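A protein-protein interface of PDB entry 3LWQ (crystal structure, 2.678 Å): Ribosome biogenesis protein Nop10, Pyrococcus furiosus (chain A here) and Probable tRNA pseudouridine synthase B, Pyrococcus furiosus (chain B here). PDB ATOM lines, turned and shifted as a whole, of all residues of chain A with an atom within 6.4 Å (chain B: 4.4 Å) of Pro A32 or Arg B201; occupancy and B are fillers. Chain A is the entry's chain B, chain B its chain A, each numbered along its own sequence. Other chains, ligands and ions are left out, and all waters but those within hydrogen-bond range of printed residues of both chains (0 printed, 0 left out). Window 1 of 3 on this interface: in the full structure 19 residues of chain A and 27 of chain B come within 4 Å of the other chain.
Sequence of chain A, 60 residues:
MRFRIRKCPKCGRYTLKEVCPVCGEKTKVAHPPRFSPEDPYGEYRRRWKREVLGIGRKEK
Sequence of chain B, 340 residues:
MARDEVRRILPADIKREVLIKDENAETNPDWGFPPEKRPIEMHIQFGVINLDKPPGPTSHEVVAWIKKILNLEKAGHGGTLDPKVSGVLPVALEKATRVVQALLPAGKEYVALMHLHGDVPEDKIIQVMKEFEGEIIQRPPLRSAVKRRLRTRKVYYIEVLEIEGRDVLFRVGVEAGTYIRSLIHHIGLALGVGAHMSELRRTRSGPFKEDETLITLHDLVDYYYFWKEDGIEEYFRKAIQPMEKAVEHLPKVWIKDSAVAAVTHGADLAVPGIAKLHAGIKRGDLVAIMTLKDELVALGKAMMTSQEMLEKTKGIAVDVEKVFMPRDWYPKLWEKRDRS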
ATOM      1  N   ILE A   5     -12.009 -25.924  25.548  1.00  0.00           N
ATOM      2  CA  ILE A   5     -12.027 -25.638  26.981  1.00  0.00           C
ATOM      3  C   ILE A   5     -13.391 -25.095  27.415  1.00  0.00           C
ATOM      4  O   ILE A   5     -13.933 -24.171  26.801  1.00  0.00           O
ATOM      5  CB  ILE A   5     -10.947 -24.637  27.381  1.00  0.00           C
ATOM      6  CG1 ILE A   5      -9.553 -25.223  27.181  1.00  0.00           C
ATOM      7  CG2 ILE A   5     -11.114 -24.227  28.841  1.00  0.00           C
ATOM      8  CD1 ILE A   5      -8.452 -24.252  27.622  1.00  0.00           C
ATOM      9  N   LYS A   7     -16.444 -24.441  30.832  1.00  0.00           N
ATOM     10  CA  LYS A   7     -16.548 -23.915  32.186  1.00  0.00           C
ATOM     11  C   LYS A   7     -17.959 -24.078  32.792  1.00  0.00           C
ATOM     12  O   LYS A   7     -18.958 -23.764  32.145  1.00  0.00           O
ATOM     13  CB  LYS A   7     -16.108 -22.447  32.171  1.00  0.00           C
ATOM     14  CG  LYS A   7     -15.493 -21.970  33.470  1.00  0.00           C
ATOM     15  CD  LYS A   7     -15.458 -20.457  33.535  1.00  0.00           C
ATOM     16  CE  LYS A   7     -14.949 -19.978  34.885  1.00  0.00           C
ATOM     17  NZ  LYS A   7     -15.167 -18.517  34.975  1.00  0.00           N
ATOM     18  N   TYR A  14     -13.150 -25.487  35.393  1.00  0.00           N
ATOM     19  CA  TYR A  14     -12.722 -25.667  34.003  1.00  0.00           C
ATOM     20  C   TYR A  14     -12.644 -27.140  33.627  1.00  0.00           C
ATOM     21  O   TYR A  14     -12.187 -27.975  34.402  1.00  0.00           O
ATOM     22  CB  TYR A  14     -11.379 -24.993  33.760  1.00  0.00           C
ATOM     23  CG  TYR A  14     -11.501 -23.534  33.449  1.00  0.00           C
ATOM     24  CD1 TYR A  14     -11.257 -22.566  34.421  1.00  0.00           C
ATOM     25  CD2 TYR A  14     -11.875 -23.116  32.181  1.00  0.00           C
ATOM     26  CE1 TYR A  14     -11.371 -21.216  34.121  1.00  0.00           C
ATOM     27  CE2 TYR A  14     -11.996 -21.781  31.873  1.00  0.00           C
ATOM     28  CZ  TYR A  14     -11.744 -20.835  32.837  1.00  0.00           C
ATOM     29  OH  TYR A  14     -11.871 -19.503  32.500  1.00  0.00           O
ATOM     30  N   VAL A  29     -18.353 -22.924  26.650  1.00  0.00           N
ATOM     31  CA  VAL A  29     -17.041 -22.622  26.108  1.00  0.00           C
ATOM     32  C   VAL A  29     -16.389 -21.440  26.789  1.00  0.00           C
ATOM     33  O   VAL A  29     -16.956 -20.359  26.843  1.00  0.00           O
ATOM     34  CB  VAL A  29     -17.136 -22.344  24.616  1.00  0.00           C
ATOM     35  CG1 VAL A  29     -15.848 -21.696  24.116  1.00  0.00           C
ATOM     36  CG2 VAL A  29     -17.439 -23.647  23.887  1.00  0.00           C
ATOM     37  N   ALA A  30     -15.183 -21.655  27.304  1.00  0.00           N
ATOM     38  CA  ALA A  30     -14.477 -20.645  28.088  1.00  0.00           C
ATOM     39  C   ALA A  30     -14.170 -19.354  27.335  1.00  0.00           C
ATOM     40  O   ALA A  30     -13.980 -18.310  27.939  1.00  0.00           O
ATOM     41  CB  ALA A  30     -13.185 -21.236  28.659  1.00  0.00           C
ATOM     42  N   HIS A  31     -14.111 -19.413  26.017  1.00  0.00           N
ATOM     43  CA  HIS A  31     -13.689 -18.247  25.272  1.00  0.00           C
ATOM     44  C   HIS A  31     -14.808 -17.277  24.983  1.00  0.00           C
ATOM     45  O   HIS A  31     -15.928 -17.684  24.709  1.00  0.00           O
ATOM     46  CB  HIS A  31     -13.007 -18.684  23.995  1.00  0.00           C
ATOM     47  CG  HIS A  31     -11.766 -19.468  24.247  1.00  0.00           C
ATOM     48  ND1 HIS A  31     -10.515 -18.889  24.269  1.00  0.00           N
ATOM     49  CD2 HIS A  31     -11.586 -20.776  24.549  1.00  0.00           C
ATOM     50  CE1 HIS A  31      -9.612 -19.814  24.545  1.00  0.00           C
ATOM     51  NE2 HIS A  31     -10.236 -20.968  24.720  1.00  0.00           N
ATOM     52  N   PRO A  32     -14.506 -15.978  25.059  1.00  0.00           N
ATOM     53  CA  PRO A  32     -15.422 -14.915  24.625  1.00  0.00           C
ATOM     54  C   PRO A  32     -15.614 -15.014  23.127  1.00  0.00           C
ATOM     55  O   PRO A  32     -14.688 -15.443  22.434  1.00  0.00           O
ATOM     56  CB  PRO A  32     -14.645 -13.628  24.921  1.00  0.00           C
ATOM     57  CG  PRO A  32     -13.581 -14.010  25.852  1.00  0.00           C
ATOM     58  CD  PRO A  32     -13.249 -15.445  25.605  1.00  0.00           C
ATOM     59  N   PRO A  33     -16.799 -14.628  22.632  1.00  0.00           N
ATOM     60  CA  PRO A  33     -17.093 -14.548  21.191  1.00  0.00           C
ATOM     61  C   PRO A  33     -16.138 -13.608  20.474  1.00  0.00           C
ATOM     62  O   PRO A  33     -15.700 -12.610  21.053  1.00  0.00           O
ATOM     63  CB  PRO A  33     -18.502 -13.966  21.148  1.00  0.00           C
ATOM     64  CG  PRO A  33     -19.105 -14.385  22.447  1.00  0.00           C
ATOM     65  CD  PRO A  33     -17.994 -14.392  23.458  1.00  0.00           C
ATOM     66  N   ARG A  34     -15.828 -13.932  19.225  1.00  0.00           N
ATOM     67  CA  ARG A  34     -14.927 -13.121  18.428  1.00  0.00           C
ATOM     68  C   ARG A  34     -15.601 -11.814  18.064  1.00  0.00           C
ATOM     69  O   ARG A  34     -16.814 -11.758  17.854  1.00  0.00           O
ATOM     70  CB  ARG A  34     -14.453 -13.900  17.188  1.00  0.00           C
ATOM     71  CG  ARG A  34     -13.282 -14.862  17.479  1.00  0.00           C
ATOM     72  CD  ARG A  34     -12.875 -15.655  16.254  1.00  0.00           C
ATOM     73  NE  ARG A  34     -11.427 -15.881  16.181  1.00  0.00           N
ATOM     74  CZ  ARG A  34     -10.806 -16.977  16.618  1.00  0.00           C
ATOM     75  NH1 ARG A  34     -11.508 -17.954  17.177  1.00  0.00           N
ATOM     76  NH2 ARG A  34      -9.484 -17.092  16.496  1.00  0.00           N
ATOM     77  N   ASP B  52     -11.924  -9.286  29.083  1.00  0.00           N
ATOM     78  CA  ASP B  52     -11.798 -10.654  28.640  1.00  0.00           C
ATOM     79  C   ASP B  52     -11.494 -10.641  27.139  1.00  0.00           C
ATOM     80  O   ASP B  52     -12.400 -10.601  26.305  1.00  0.00           O
ATOM     81  CB  ASP B  52     -13.122 -11.386  28.908  1.00  0.00           C
ATOM     82  CG  ASP B  52     -13.033 -12.900  28.674  1.00  0.00           C
ATOM     83  OD1 ASP B  52     -11.941 -13.402  28.301  1.00  0.00           O
ATOM     84  OD2 ASP B  52     -14.073 -13.582  28.866  1.00  0.00           O
ATOM     85  N   LYS B  53     -10.210 -10.657  26.806  1.00  0.00           N
ATOM     86  CA  LYS B  53      -9.772 -10.630  25.424  1.00  0.00           C
ATOM     87  C   LYS B  53     -10.287 -11.845  24.629  1.00  0.00           C
ATOM     88  O   LYS B  53     -10.226 -12.986  25.090  1.00  0.00           O
ATOM     89  CB  LYS B  53      -8.249 -10.559  25.382  1.00  0.00           C
ATOM     90  CG  LYS B  53      -7.664 -10.454  23.993  1.00  0.00           C
ATOM     91  CD  LYS B  53      -6.155 -10.666  24.010  1.00  0.00           C
ATOM     92  CE  LYS B  53      -5.633 -10.938  22.603  1.00  0.00           C
ATOM     93  NZ  LYS B  53      -6.201 -12.221  22.072  1.00  0.00           N
ATOM     94  N   PRO B  54     -10.800 -11.598  23.418  1.00  0.00           N
ATOM     95  CA  PRO B  54     -11.226 -12.681  22.523  1.00  0.00           C
ATOM     96  C   PRO B  54     -10.035 -13.320  21.805  1.00  0.00           C
ATOM     97  O   PRO B  54      -8.988 -12.701  21.650  1.00  0.00           O
ATOM     98  CB  PRO B  54     -12.100 -11.963  21.491  1.00  0.00           C
ATOM     99  CG  PRO B  54     -12.224 -10.540  21.970  1.00  0.00           C
ATOM    100  CD  PRO B  54     -11.053 -10.276  22.837  1.00  0.00           C
ATOM    101  N   PRO B  55     -10.188 -14.578  21.402  1.00  0.00           N
ATOM    102  CA  PRO B  55      -9.277 -15.219  20.456  1.00  0.00           C
ATOM    103  C   PRO B  55      -9.217 -14.409  19.162  1.00  0.00           C
ATOM    104  O   PRO B  55     -10.260 -13.982  18.672  1.00  0.00           O
ATOM    105  CB  PRO B  55      -9.960 -16.557  20.185  1.00  0.00           C
ATOM    106  CG  PRO B  55     -10.732 -16.848  21.447  1.00  0.00           C
ATOM    107  CD  PRO B  55     -11.219 -15.503  21.910  1.00  0.00           C
ATOM    108  N   VAL B  85      -4.553 -16.434  22.401  1.00  0.00           N
ATOM    109  CA  VAL B  85      -4.949 -16.514  23.813  1.00  0.00           C
ATOM    110  C   VAL B  85      -6.079 -15.553  24.212  1.00  0.00           C
ATOM    111  O   VAL B  85      -6.181 -14.434  23.700  1.00  0.00           O
ATOM    112  CB  VAL B  85      -3.713 -16.288  24.742  1.00  0.00           C
ATOM    113  CG1 VAL B  85      -4.045 -16.578  26.205  1.00  0.00           C
ATOM    114  CG2 VAL B  85      -2.520 -17.142  24.288  1.00  0.00           C
ATOM    115  N   SER B  86      -6.922 -15.995  25.141  1.00  0.00           N
ATOM    116  CA  SER B  86      -8.039 -15.178  25.628  1.00  0.00           C
ATOM    117  C   SER B  86      -7.854 -14.823  27.103  1.00  0.00           C
ATOM    118  O   SER B  86      -6.839 -15.178  27.719  1.00  0.00           O
ATOM    119  CB  SER B  86      -9.360 -15.944  25.494  1.00  0.00           C
ATOM    120  OG  SER B  86      -9.405 -16.990  26.464  1.00  0.00           O
ATOM    121  N   GLY B  87      -8.849 -14.121  27.653  1.00  0.00           N
ATOM    122  CA  GLY B  87      -8.968 -13.919  29.081  1.00  0.00           C
ATOM    123  C   GLY B  87      -8.511 -12.574  29.604  1.00  0.00           C
ATOM    124  O   GLY B  87      -8.307 -11.644  28.838  1.00  0.00           O
ATOM    125  N   GLU B 109      -2.216 -16.168  36.451  1.00  0.00           N
ATOM    126  CA  GLU B 109      -2.738 -17.529  36.407  1.00  0.00           C
ATOM    127  C   GLU B 109      -3.307 -17.878  35.013  1.00  0.00           C
ATOM    128  O   GLU B 109      -3.986 -17.061  34.387  1.00  0.00           O
ATOM    129  CB  GLU B 109      -3.780 -17.748  37.496  1.00  0.00           C
ATOM    130  CG  GLU B 109      -4.244 -19.192  37.609  1.00  0.00           C
ATOM    131  CD  GLU B 109      -5.394 -19.376  38.597  1.00  0.00           C
ATOM    132  OE1 GLU B 109      -5.705 -20.544  38.925  1.00  0.00           O
ATOM    133  OE2 GLU B 109      -5.981 -18.366  39.046  1.00  0.00           O
ATOM    134  N   TYR B 110      -3.017 -19.086  34.524  1.00  0.00           N
ATOM    135  CA  TYR B 110      -3.595 -19.550  33.257  1.00  0.00           C
ATOM    136  C   TYR B 110      -4.319 -20.879  33.401  1.00  0.00           C
ATOM    137  O   TYR B 110      -4.069 -21.641  34.340  1.00  0.00           O
ATOM    138  CB  TYR B 110      -2.524 -19.692  32.166  1.00  0.00           C
ATOM    139  CG  TYR B 110      -1.739 -18.432  31.882  1.00  0.00           C
ATOM    140  CD1 TYR B 110      -0.617 -18.119  32.626  1.00  0.00           C
ATOM    141  CD2 TYR B 110      -2.118 -17.559  30.879  1.00  0.00           C
ATOM    142  CE1 TYR B 110       0.120 -16.979  32.378  1.00  0.00           C
ATOM    143  CE2 TYR B 110      -1.382 -16.408  30.624  1.00  0.00           C
ATOM    144  CZ  TYR B 110      -0.262 -16.123  31.386  1.00  0.00           C
ATOM    145  OH  TYR B 110       0.487 -14.980  31.168  1.00  0.00           O
ATOM    146  N   VAL B 111      -5.226 -21.149  32.471  1.00  0.00           N
ATOM    147  CA  VAL B 111      -5.701 -22.514  32.273  1.00  0.00           C
ATOM    148  C   VAL B 111      -5.239 -22.887  30.883  1.00  0.00           C
ATOM    149  O   VAL B 111      -5.500 -22.163  29.923  1.00  0.00           O
ATOM    150  CB  VAL B 111      -7.220 -22.634  32.392  1.00  0.00           C
ATOM    151  CG1 VAL B 111      -7.703 -23.822  31.648  1.00  0.00           C
ATOM    152  CG2 VAL B 111      -7.623 -22.749  33.851  1.00  0.00           C
ATOM    153  N   LEU B 200      -4.883 -21.654  25.292  1.00  0.00           N
ATOM    154  CA  LEU B 200      -4.481 -20.924  26.493  1.00  0.00           C
ATOM    155  C   LEU B 200      -5.481 -19.852  26.884  1.00  0.00           C
ATOM    156  O   LEU B 200      -5.987 -19.122  26.038  1.00  0.00           O
ATOM    157  CB  LEU B 200      -3.119 -20.271  26.305  1.00  0.00           C
ATOM    158  CG  LEU B 200      -2.451 -19.850  27.615  1.00  0.00           C
ATOM    159  CD1 LEU B 200      -2.253 -21.070  28.497  1.00  0.00           C
ATOM    160  CD2 LEU B 200      -1.112 -19.114  27.360  1.00  0.00           C
ATOM    161  N   ARG B 201      -5.753 -19.748  28.179  1.00  0.00           N
ATOM    162  CA  ARG B 201      -6.605 -18.682  28.688  1.00  0.00           C
ATOM    163  C   ARG B 201      -6.063 -18.144  30.004  1.00  0.00           C
ATOM    164  O   ARG B 201      -5.830 -18.919  30.949  1.00  0.00           O
ATOM    165  CB  ARG B 201      -8.023 -19.210  28.885  1.00  0.00           C
ATOM    166  CG  ARG B 201      -8.924 -18.278  29.632  1.00  0.00           C
ATOM    167  CD  ARG B 201     -10.355 -18.659  29.434  1.00  0.00           C
ATOM    168  NE  ARG B 201     -11.222 -17.716  30.123  1.00  0.00           N
ATOM    169  CZ  ARG B 201     -11.784 -16.651  29.558  1.00  0.00           C
ATOM    170  NH1 ARG B 201     -11.597 -16.373  28.268  1.00  0.00           N
ATOM    171  NH2 ARG B 201     -12.558 -15.865  30.289  1.00  0.00           N
ATOM    172  N   ARG B 202      -5.854 -16.830  30.066  1.00  0.00           N
ATOM    173  CA  ARG B 202      -5.446 -16.190  31.326  1.00  0.00           C
ATOM    174  C   ARG B 202      -6.652 -15.887  32.208  1.00  0.00           C
ATOM    175  O   ARG B 202      -7.593 -15.239  31.770  1.00  0.00           O
ATOM    176  CB  ARG B 202      -4.660 -14.915  31.078  1.00  0.00           C
ATOM    177  CG  ARG B 202      -4.012 -14.362  32.333  1.00  0.00           C
ATOM    178  CD  ARG B 202      -3.772 -12.901  32.180  1.00  0.00           C
ATOM    179  NE  ARG B 202      -2.454 -12.601  31.660  1.00  0.00           N
ATOM    180  CZ  ARG B 202      -2.158 -11.490  31.000  1.00  0.00           C
ATOM    181  NH1 ARG B 202      -3.098 -10.590  30.749  1.00  0.00           N
ATOM    182  NH2 ARG B 202      -0.924 -11.288  30.578  1.00  0.00           N
ATOM    183  N   THR B 203      -6.591 -16.364  33.449  1.00  0.00           N
ATOM    184  CA  THR B 203      -7.705 -16.352  34.395  1.00  0.00           C
ATOM    185  C   THR B 203      -7.502 -15.320  35.528  1.00  0.00           C
ATOM    186  O   THR B 203      -8.413 -15.045  36.315  1.00  0.00           O
ATOM    187  CB  THR B 203      -7.828 -17.734  35.092  1.00  0.00           C
ATOM    188  OG1 THR B 203      -6.532 -18.165  35.521  1.00  0.00           O
ATOM    189  CG2 THR B 203      -8.399 -18.787  34.172  1.00  0.00           C
ATOM    190  N   GLU B 210     -11.281 -13.610  37.203  1.00  0.00           N
ATOM    191  CA  GLU B 210     -12.547 -13.847  36.521  1.00  0.00           C
ATOM    192  C   GLU B 210     -13.681 -13.686  37.522  1.00  0.00           C
ATOM    193  O   GLU B 210     -13.967 -14.606  38.292  1.00  0.00           O
ATOM    194  CB  GLU B 210     -12.603 -15.252  35.934  1.00  0.00           C
ATOM    195  CG  GLU B 210     -11.945 -15.419  34.566  1.00  0.00           C
ATOM    196  CD  GLU B 210     -12.118 -16.832  34.014  1.00  0.00           C
ATOM    197  OE1 GLU B 210     -11.313 -17.713  34.382  1.00  0.00           O
ATOM    198  OE2 GLU B 210     -13.066 -17.061  33.226  1.00  0.00           O
ATOM    199  N   LEU B 214     -15.337  -8.947  35.167  1.00  0.00           N
ATOM    200  CA  LEU B 214     -14.711  -9.397  33.924  1.00  0.00           C
ATOM    201  C   LEU B 214     -15.672  -9.315  32.752  1.00  0.00           C
ATOM    202  O   LEU B 214     -16.631 -10.079  32.679  1.00  0.00           O
ATOM    203  CB  LEU B 214     -14.189 -10.826  34.055  1.00  0.00           C
ATOM    204  CG  LEU B 214     -13.407 -11.283  32.824  1.00  0.00           C
ATOM    205  CD1 LEU B 214     -11.979 -10.752  32.895  1.00  0.00           C
ATOM    206  CD2 LEU B 214     -13.431 -12.802  32.667  1.00  0.00           C
ATOM    207  N   THR B 216     -16.596  -8.785  28.466  1.00  0.00           N
ATOM    208  CA  THR B 216     -16.269  -8.940  27.048  1.00  0.00           C
ATOM    209  C   THR B 216     -16.414  -7.639  26.284  1.00  0.00           C
ATOM    210  O   THR B 216     -17.024  -6.688  26.777  1.00  0.00           O
ATOM    211  CB  THR B 216     -17.236  -9.900  26.382  1.00  0.00           C
ATOM    212  OG1 THR B 216     -18.554  -9.335  26.422  1.00  0.00           O
ATOM    213  CG2 THR B 216     -17.236 -11.237  27.088  1.00  0.00           C
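O of Pro B55 is in hydrogen-bond range of NE of Arg A34 (3.3 Å). The side-chain hydroxyl (OG) of Ser B86 is in hydrogen-bond range of a ring nitrogen (ND1) of His A31. NE of Arg B201 lies within hydrogen-bond range of OH of Tyr A14 (3.0 Å). NH1 of Arg B201 sits at hydrogen-bond distance from O of Ala A30 (3.1 Å). The side-chain carboxylate of Glu B210 is in salt-bridge range of the side-chain amino group of Lys A7 (3.1 Å). OE1 of Glu B210 sits at hydrogen-bond distance from OH of Tyr A14.
N of Gly B87 lies close to OD1 of Asp B52 (3.2 Å). NH1 of Arg B201 lies within salt-bridge range of OD1 of Asp B52, at 3.0 Å. NZ of Lys B53 lies within hydrogen-bond range of O of Val B85, at 2.7 Å. The backbone carbonyl oxygen (O) of Gly B87 lies within hydrogen-bond range of the backbone NH (N) of Lys B53, 3.0 Å away. The side-chain hydroxyl of Ser B86 is in hydrogen-bond range of the guanidinium group of Arg B201. The backbone carbonyl oxygen (O) of Thr B203 sits at hydrogen-bond distance from the backbone NH (N) of Glu B210, 3.3 Å away.
Tyr A14 touches Val B111 (CD1 to CG2, 3.7 Å). Tyr A14 touches Thr B203. His A31 touches Pro B55. Leu B200 touches His A31 (O to CE1, 3.98 Å). Asp B52 touches Pro A32 (OD1 to CG, 3.0 Å). Lys B53 touches Pro A32 (O to CG, 3.6 Å). Pro B55 touches Pro A32. CB of Ser B86 touches CD of Pro A32 (3.9 Å). Pro A32 touches Arg B201. Pro A33 touches Pro B54.
Ile A5 touches none of the printed residues of chain B. Printed residues of chain B within 4 Å of Tyr A14: Val B111 (3.7 Å), Arg B201 (3.0 Å), Thr B203 (3.8 Å) and Glu B210 (2.7 Å). Pro A32 touches just these residues of chain B: Asp B52 (3.0 Å), Lys B53 (3.6 Å), Pro B55 (3.5 Å), Ser B86 (3.9 Å) and Arg B201 (3.3 Å). Of the printed residues of chain B, Pro A33 touches Pro B54 (3.7 Å). Of the printed residues of chain A, Ser B86 touches His A31 (3.1 Å) and Pro A32 (3.9 Å). Arg B201 touches just these residues of chain A: Tyr A14, Ala A30 and Pro A32. The nearest residue of chain A that does not touch Arg B201 is His A31 (4.1 Å).
Of the 9 printed residues of chain A, 7 touch a printed residue of chain B. Printed residues of chain A that touch a printed residue of chain B: Lys A7, Tyr A14, Ala A30, His A31, Pro A32, Pro A33 and Arg A34. Hydrophobic or aromatic side chains of chain A within 4 Å of the printed part of chain B: Tyr A14, Ala A30, His A31 and Pro A32. Of the 17 printed residues of chain B, 10 touch a printed residue of chain A. Hydrophobic or aromatic side chains of chain B within 4 Å of the printed part of chain A: Pro B54, Pro B55 and Val B111.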
